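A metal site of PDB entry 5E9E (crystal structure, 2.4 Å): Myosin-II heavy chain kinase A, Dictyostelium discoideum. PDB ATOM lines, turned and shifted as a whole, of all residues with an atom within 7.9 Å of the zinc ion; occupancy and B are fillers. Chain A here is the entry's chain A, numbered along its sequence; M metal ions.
The zinc ion is bound by ND1 of His 208 (2.1 Å). The zinc ion is bound by NE2 of His 260 (2.1 Å). The zinc ion is bound by the side-chain sulfur (SG) of Cys 266, 2.2 Å away. The side-chain sulfur (SG) of Cys 262 binds the zinc ion, 2.4 Å away. The zinc ion has four donor atoms within binding distance.
Within 4 Å of the zinc ion: His 208, His 260, Cys 262 and Cys 266. The nearest printed residue that does not touch the zinc ion is Leu 271 (4.4 Å).
The backbone NH of Leu 271 lies within hydrogen-bond range of the backbone carbonyl oxygen of Cys 266, at 3.1 Å. The backbone NH (N) of Cys 266 lies within hydrogen-bond range of the side-chain amide oxygen (OD1) of Asn 263, 3.0 Å away. The backbone carbonyl oxygen (O) of Asp 272 lies close to the side-chain sulfur (SG) of Cys 262. N of Cys 262 lies within hydrogen-bond range of O of Lys 274 (3.1 Å).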
ATOM      1  N   SER A 201     -19.705  18.440 -22.770  1.00  0.00           N
ATOM      2  CA  SER A 201     -19.850  17.360 -21.811  1.00  0.00           C
ATOM      3  C   SER A 201     -21.234  16.663 -21.855  1.00  0.00           C
ATOM      4  O   SER A 201     -21.332  15.418 -21.818  1.00  0.00           O
ATOM      5  CB  SER A 201     -19.632  17.911 -20.386  1.00  0.00           C
ATOM      6  OG  SER A 201     -18.267  18.082 -20.108  1.00  0.00           O
ATOM      7  N   GLN A 204     -22.017  13.612 -24.136  1.00  0.00           N
ATOM      8  CA  GLN A 204     -21.277  12.385 -23.856  1.00  0.00           C
ATOM      9  C   GLN A 204     -21.753  11.787 -22.566  1.00  0.00           C
ATOM     10  O   GLN A 204     -21.885  10.578 -22.445  1.00  0.00           O
ATOM     11  CB  GLN A 204     -19.759  12.652 -23.768  1.00  0.00           C
ATOM     12  CG  GLN A 204     -19.162  13.418 -24.938  1.00  0.00           C
ATOM     13  CD  GLN A 204     -19.487  12.787 -26.266  1.00  0.00           C
ATOM     14  OE1 GLN A 204     -19.554  11.565 -26.392  1.00  0.00           O
ATOM     15  NE2 GLN A 204     -19.678  13.613 -27.268  1.00  0.00           N
ATOM     16  N   ALA A 205     -22.018  12.634 -21.585  1.00  0.00           N
ATOM     17  CA  ALA A 205     -22.546  12.188 -20.327  1.00  0.00           C
ATOM     18  C   ALA A 205     -23.948  11.590 -20.519  1.00  0.00           C
ATOM     19  O   ALA A 205     -24.345  10.663 -19.807  1.00  0.00           O
ATOM     20  CB  ALA A 205     -22.580  13.337 -19.334  1.00  0.00           C
ATOM     21  N   PHE A 206     -24.703  12.100 -21.481  1.00  0.00           N
ATOM     22  CA  PHE A 206     -26.015  11.522 -21.757  1.00  0.00           C
ATOM     23  C   PHE A 206     -25.830  10.133 -22.336  1.00  0.00           C
ATOM     24  O   PHE A 206     -26.457   9.187 -21.892  1.00  0.00           O
ATOM     25  CB  PHE A 206     -26.850  12.386 -22.695  1.00  0.00           C
ATOM     26  CG  PHE A 206     -28.101  11.695 -23.184  1.00  0.00           C
ATOM     27  CD1 PHE A 206     -29.141  11.448 -22.309  1.00  0.00           C
ATOM     28  CD2 PHE A 206     -28.214  11.251 -24.475  1.00  0.00           C
ATOM     29  CE1 PHE A 206     -30.293  10.787 -22.735  1.00  0.00           C
ATOM     30  CE2 PHE A 206     -29.353  10.590 -24.908  1.00  0.00           C
ATOM     31  CZ  PHE A 206     -30.390  10.348 -24.042  1.00  0.00           C
ATOM     32  N   SER A 207     -24.944  10.002 -23.321  1.00  0.00           N
ATOM     33  CA  SER A 207     -24.698   8.705 -23.906  1.00  0.00           C
ATOM     34  C   SER A 207     -24.301   7.731 -22.811  1.00  0.00           C
ATOM     35  O   SER A 207     -24.839   6.613 -22.722  1.00  0.00           O
ATOM     36  CB  SER A 207     -23.641   8.797 -24.959  1.00  0.00           C
ATOM     37  OG  SER A 207     -24.171   9.455 -26.094  1.00  0.00           O
ATOM     38  N   HIS A 208     -23.402   8.169 -21.954  1.00  0.00           N
ATOM     39  CA  HIS A 208     -22.908   7.316 -20.874  1.00  0.00           C
ATOM     40  C   HIS A 208     -24.062   6.929 -19.941  1.00  0.00           C
ATOM     41  O   HIS A 208     -24.269   5.753 -19.649  1.00  0.00           O
ATOM     42  CB  HIS A 208     -21.762   7.987 -20.121  1.00  0.00           C
ATOM     43  CG  HIS A 208     -21.104   7.094 -19.123  1.00  0.00           C
ATOM     44  ND1 HIS A 208     -20.146   7.552 -18.247  1.00  0.00           N
ATOM     45  CD2 HIS A 208     -21.254   5.776 -18.861  1.00  0.00           C
ATOM     46  CE1 HIS A 208     -19.761   6.555 -17.467  1.00  0.00           C
ATOM     47  NE2 HIS A 208     -20.409   5.468 -17.822  1.00  0.00           N
ATOM     48  N   PHE A 209     -24.825   7.933 -19.507  1.00  0.00           N
ATOM     49  CA  PHE A 209     -26.025   7.728 -18.685  1.00  0.00           C
ATOM     50  C   PHE A 209     -26.885   6.588 -19.236  1.00  0.00           C
ATOM     51  O   PHE A 209     -27.260   5.676 -18.498  1.00  0.00           O
ATOM     52  CB  PHE A 209     -26.832   9.039 -18.675  1.00  0.00           C
ATOM     53  CG  PHE A 209     -28.120   8.981 -17.880  1.00  0.00           C
ATOM     54  CD1 PHE A 209     -28.103   9.122 -16.504  1.00  0.00           C
ATOM     55  CD2 PHE A 209     -29.332   8.848 -18.523  1.00  0.00           C
ATOM     56  CE1 PHE A 209     -29.281   9.090 -15.770  1.00  0.00           C
ATOM     57  CE2 PHE A 209     -30.513   8.828 -17.809  1.00  0.00           C
ATOM     58  CZ  PHE A 209     -30.489   8.937 -16.421  1.00  0.00           C
ATOM     59  N   GLU A 212     -25.148   3.105 -18.770  1.00  0.00           N
ATOM     60  CA  GLU A 212     -25.196   2.560 -17.421  1.00  0.00           C
ATOM     61  C   GLU A 212     -26.619   2.279 -16.960  1.00  0.00           C
ATOM     62  O   GLU A 212     -26.900   1.192 -16.448  1.00  0.00           O
ATOM     63  CB  GLU A 212     -24.501   3.480 -16.428  1.00  0.00           C
ATOM     64  CG  GLU A 212     -24.479   2.924 -15.012  1.00  0.00           C
ATOM     65  CD  GLU A 212     -23.543   3.662 -14.055  1.00  0.00           C
ATOM     66  OE1 GLU A 212     -23.898   3.775 -12.854  1.00  0.00           O
ATOM     67  OE2 GLU A 212     -22.447   4.121 -14.491  1.00  0.00           O
ATOM     68  N   PHE A 256     -18.396   2.778 -28.155  1.00  0.00           N
ATOM     69  CA  PHE A 256     -18.720   4.000 -27.436  1.00  0.00           C
ATOM     70  C   PHE A 256     -17.965   4.032 -26.131  1.00  0.00           C
ATOM     71  O   PHE A 256     -17.314   5.037 -25.799  1.00  0.00           O
ATOM     72  CB  PHE A 256     -20.208   4.150 -27.098  1.00  0.00           C
ATOM     73  CG  PHE A 256     -20.437   5.232 -26.092  1.00  0.00           C
ATOM     74  CD1 PHE A 256     -20.409   6.570 -26.473  1.00  0.00           C
ATOM     75  CD2 PHE A 256     -20.496   4.928 -24.746  1.00  0.00           C
ATOM     76  CE1 PHE A 256     -20.521   7.583 -25.535  1.00  0.00           C
ATOM     77  CE2 PHE A 256     -20.601   5.925 -23.823  1.00  0.00           C
ATOM     78  CZ  PHE A 256     -20.618   7.257 -24.212  1.00  0.00           C
ATOM     79  N   ILE A 257     -18.087   2.940 -25.376  1.00  0.00           N
ATOM     80  CA  ILE A 257     -17.617   2.944 -24.017  1.00  0.00           C
ATOM     81  C   ILE A 257     -16.097   2.991 -24.002  1.00  0.00           C
ATOM     82  O   ILE A 257     -15.545   3.639 -23.125  1.00  0.00           O
ATOM     83  CB  ILE A 257     -18.255   1.842 -23.115  1.00  0.00           C
ATOM     84  CG1 ILE A 257     -18.125   2.237 -21.618  1.00  0.00           C
ATOM     85  CG2 ILE A 257     -17.695   0.453 -23.426  1.00  0.00           C
ATOM     86  CD1 ILE A 257     -19.073   3.333 -21.167  1.00  0.00           C
ATOM     87  N   HIS A 260     -14.835   6.691 -24.596  1.00  0.00           N
ATOM     88  CA  HIS A 260     -15.502   7.659 -23.724  1.00  0.00           C
ATOM     89  C   HIS A 260     -14.639   8.012 -22.525  1.00  0.00           C
ATOM     90  O   HIS A 260     -14.117   7.129 -21.875  1.00  0.00           O
ATOM     91  CB  HIS A 260     -16.835   7.100 -23.237  1.00  0.00           C
ATOM     92  CG  HIS A 260     -17.469   7.942 -22.177  1.00  0.00           C
ATOM     93  ND1 HIS A 260     -18.031   9.175 -22.457  1.00  0.00           N
ATOM     94  CD2 HIS A 260     -17.589   7.750 -20.850  1.00  0.00           C
ATOM     95  CE1 HIS A 260     -18.493   9.691 -21.327  1.00  0.00           C
ATOM     96  NE2 HIS A 260     -18.240   8.845 -20.345  1.00  0.00           N
ATOM     97  N   LYS A 261     -14.511   9.316 -22.259  1.00  0.00           N
ATOM     98  CA  LYS A 261     -13.835   9.871 -21.088  1.00  0.00           C
ATOM     99  C   LYS A 261     -14.866  10.620 -20.266  1.00  0.00           C
ATOM    100  O   LYS A 261     -15.505  11.559 -20.762  1.00  0.00           O
ATOM    101  CB  LYS A 261     -12.782  10.914 -21.490  1.00  0.00           C
ATOM    102  CG  LYS A 261     -11.464  10.428 -22.110  1.00  0.00           C
ATOM    103  CD  LYS A 261     -10.412  11.553 -22.060  1.00  0.00           C
ATOM    104  CE  LYS A 261      -8.971  11.081 -22.049  1.00  0.00           C
ATOM    105  NZ  LYS A 261      -8.596  10.270 -23.238  1.00  0.00           N
ATOM    106  N   CYS A 262     -15.040  10.235 -19.009  1.00  0.00           N
ATOM    107  CA  CYS A 262     -16.045  10.878 -18.202  1.00  0.00           C
ATOM    108  C   CYS A 262     -15.676  12.342 -17.993  1.00  0.00           C
ATOM    109  O   CYS A 262     -14.493  12.732 -18.010  1.00  0.00           O
ATOM    110  CB  CYS A 262     -16.258  10.159 -16.877  1.00  0.00           C
ATOM    111  SG  CYS A 262     -17.090   8.560 -17.019  1.00  0.00           S
ATOM    112  N   ASN A 263     -16.722  13.139 -17.780  1.00  0.00           N
ATOM    113  CA  ASN A 263     -16.564  14.561 -17.531  1.00  0.00           C
ATOM    114  C   ASN A 263     -17.311  14.886 -16.246  1.00  0.00           C
ATOM    115  O   ASN A 263     -17.810  13.986 -15.571  1.00  0.00           O
ATOM    116  CB  ASN A 263     -17.111  15.338 -18.723  1.00  0.00           C
ATOM    117  CG  ASN A 263     -18.573  14.986 -19.049  1.00  0.00           C
ATOM    118  OD1 ASN A 263     -19.438  14.963 -18.159  1.00  0.00           O
ATOM    119  ND2 ASN A 263     -18.831  14.662 -20.307  1.00  0.00           N
ATOM    120  N   ALA A 264     -17.411  16.163 -15.938  1.00  0.00           N
ATOM    121  CA  ALA A 264     -18.092  16.614 -14.723  1.00  0.00           C
ATOM    122  C   ALA A 264     -19.561  16.186 -14.610  1.00  0.00           C
ATOM    123  O   ALA A 264     -20.074  15.942 -13.512  1.00  0.00           O
ATOM    124  CB  ALA A 264     -17.970  18.118 -14.624  1.00  0.00           C
ATOM    125  N   VAL A 265     -20.247  16.110 -15.747  1.00  0.00           N
ATOM    126  CA  VAL A 265     -21.655  15.740 -15.771  1.00  0.00           C
ATOM    127  C   VAL A 265     -21.764  14.272 -15.409  1.00  0.00           C
ATOM    128  O   VAL A 265     -22.616  13.890 -14.604  1.00  0.00           O
ATOM    129  CB  VAL A 265     -22.316  16.044 -17.135  1.00  0.00           C
ATOM    130  CG1 VAL A 265     -23.811  15.693 -17.125  1.00  0.00           C
ATOM    131  CG2 VAL A 265     -22.152  17.510 -17.500  1.00  0.00           C
ATOM    132  N   CYS A 266     -20.895  13.434 -15.984  1.00  0.00           N
ATOM    133  CA  CYS A 266     -20.911  12.019 -15.598  1.00  0.00           C
ATOM    134  C   CYS A 266     -20.758  11.933 -14.098  1.00  0.00           C
ATOM    135  O   CYS A 266     -21.482  11.177 -13.434  1.00  0.00           O
ATOM    136  CB  CYS A 266     -19.772  11.244 -16.241  1.00  0.00           C
ATOM    137  SG  CYS A 266     -19.765  11.282 -18.038  1.00  0.00           S
ATOM    138  N   ALA A 267     -19.824  12.706 -13.566  1.00  0.00           N
ATOM    139  CA  ALA A 267     -19.574  12.689 -12.137  1.00  0.00           C
ATOM    140  C   ALA A 267     -20.805  13.173 -11.346  1.00  0.00           C
ATOM    141  O   ALA A 267     -21.200  12.539 -10.376  1.00  0.00           O
ATOM    142  CB  ALA A 267     -18.342  13.525 -11.812  1.00  0.00           C
ATOM    143  N   LEU A 271     -22.023   8.336 -12.327  1.00  0.00           N
ATOM    144  CA  LEU A 271     -21.776   7.234 -13.242  1.00  0.00           C
ATOM    145  C   LEU A 271     -20.394   6.622 -12.945  1.00  0.00           C
ATOM    146  O   LEU A 271     -19.522   7.295 -12.411  1.00  0.00           O
ATOM    147  CB  LEU A 271     -21.829   7.755 -14.685  1.00  0.00           C
ATOM    148  CG  LEU A 271     -23.120   8.420 -15.167  1.00  0.00           C
ATOM    149  CD1 LEU A 271     -22.997   8.919 -16.600  1.00  0.00           C
ATOM    150  CD2 LEU A 271     -24.322   7.470 -15.046  1.00  0.00           C
ATOM    151  N   ASP A 272     -20.210   5.361 -13.307  1.00  0.00           N
ATOM    152  CA  ASP A 272     -18.906   4.697 -13.109  1.00  0.00           C
ATOM    153  C   ASP A 272     -17.845   5.358 -13.955  1.00  0.00           C
ATOM    154  O   ASP A 272     -17.996   5.457 -15.159  1.00  0.00           O
ATOM    155  CB  ASP A 272     -18.952   3.242 -13.550  1.00  0.00           C
ATOM    156  CG  ASP A 272     -19.706   2.329 -12.608  1.00  0.00           C
ATOM    157  OD1 ASP A 272     -19.999   2.708 -11.451  1.00  0.00           O
ATOM    158  OD2 ASP A 272     -20.004   1.192 -13.061  1.00  0.00           O
ATOM    159  N   VAL A 273     -16.720   5.711 -13.363  1.00  0.00           N
ATOM    160  CA  VAL A 273     -15.733   6.522 -14.078  1.00  0.00           C
ATOM    161  C   VAL A 273     -14.932   5.719 -15.126  1.00  0.00           C
ATOM    162  O   VAL A 273     -14.441   4.631 -14.856  1.00  0.00           O
ATOM    163  CB  VAL A 273     -14.853   7.369 -13.116  1.00  0.00           C
ATOM    164  CG1 VAL A 273     -14.138   6.530 -12.073  1.00  0.00           C
ATOM    165  CG2 VAL A 273     -13.852   8.169 -13.924  1.00  0.00           C
ATOM    166  N   LYS A 274     -14.875   6.270 -16.341  1.00  0.00           N
ATOM    167  CA  LYS A 274     -14.159   5.672 -17.481  1.00  0.00           C
ATOM    168  C   LYS A 274     -13.066   6.623 -17.886  1.00  0.00           C
ATOM    169  O   LYS A 274     -13.305   7.837 -18.006  1.00  0.00           O
ATOM    170  CB  LYS A 274     -15.067   5.501 -18.686  1.00  0.00           C
ATOM    171  CG  LYS A 274     -16.381   4.769 -18.429  1.00  0.00           C
ATOM    172  CD  LYS A 274     -16.139   3.341 -17.987  1.00  0.00           C
ATOM    173  CE  LYS A 274     -17.439   2.690 -17.585  1.00  0.00           C
ATOM    174  NZ  LYS A 274     -17.224   1.443 -16.795  1.00  0.00           N
ATOM    175  N   LEU A 275     -11.897   6.073 -18.162  1.00  0.00           N
ATOM    176  CA  LEU A 275     -10.713   6.873 -18.450  1.00  0.00           C
ATOM    177  C   LEU A 275     -10.364   7.013 -19.933  1.00  0.00           C
ATOM    178  O   LEU A 275      -9.448   7.752 -20.267  1.00  0.00           O
ATOM    179  CB  LEU A 275      -9.539   6.321 -17.638  1.00  0.00           C
ATOM    180  CG  LEU A 275      -9.658   6.647 -16.139  1.00  0.00           C
ATOM    181  CD1 LEU A 275      -8.710   5.794 -15.303  1.00  0.00           C
ATOM    182  CD2 LEU A 275      -9.415   8.121 -15.881  1.00  0.00           C
HETATM  183 ZN    ZN M   1     -18.973   9.257 -18.392  1.00  0.00          ZN
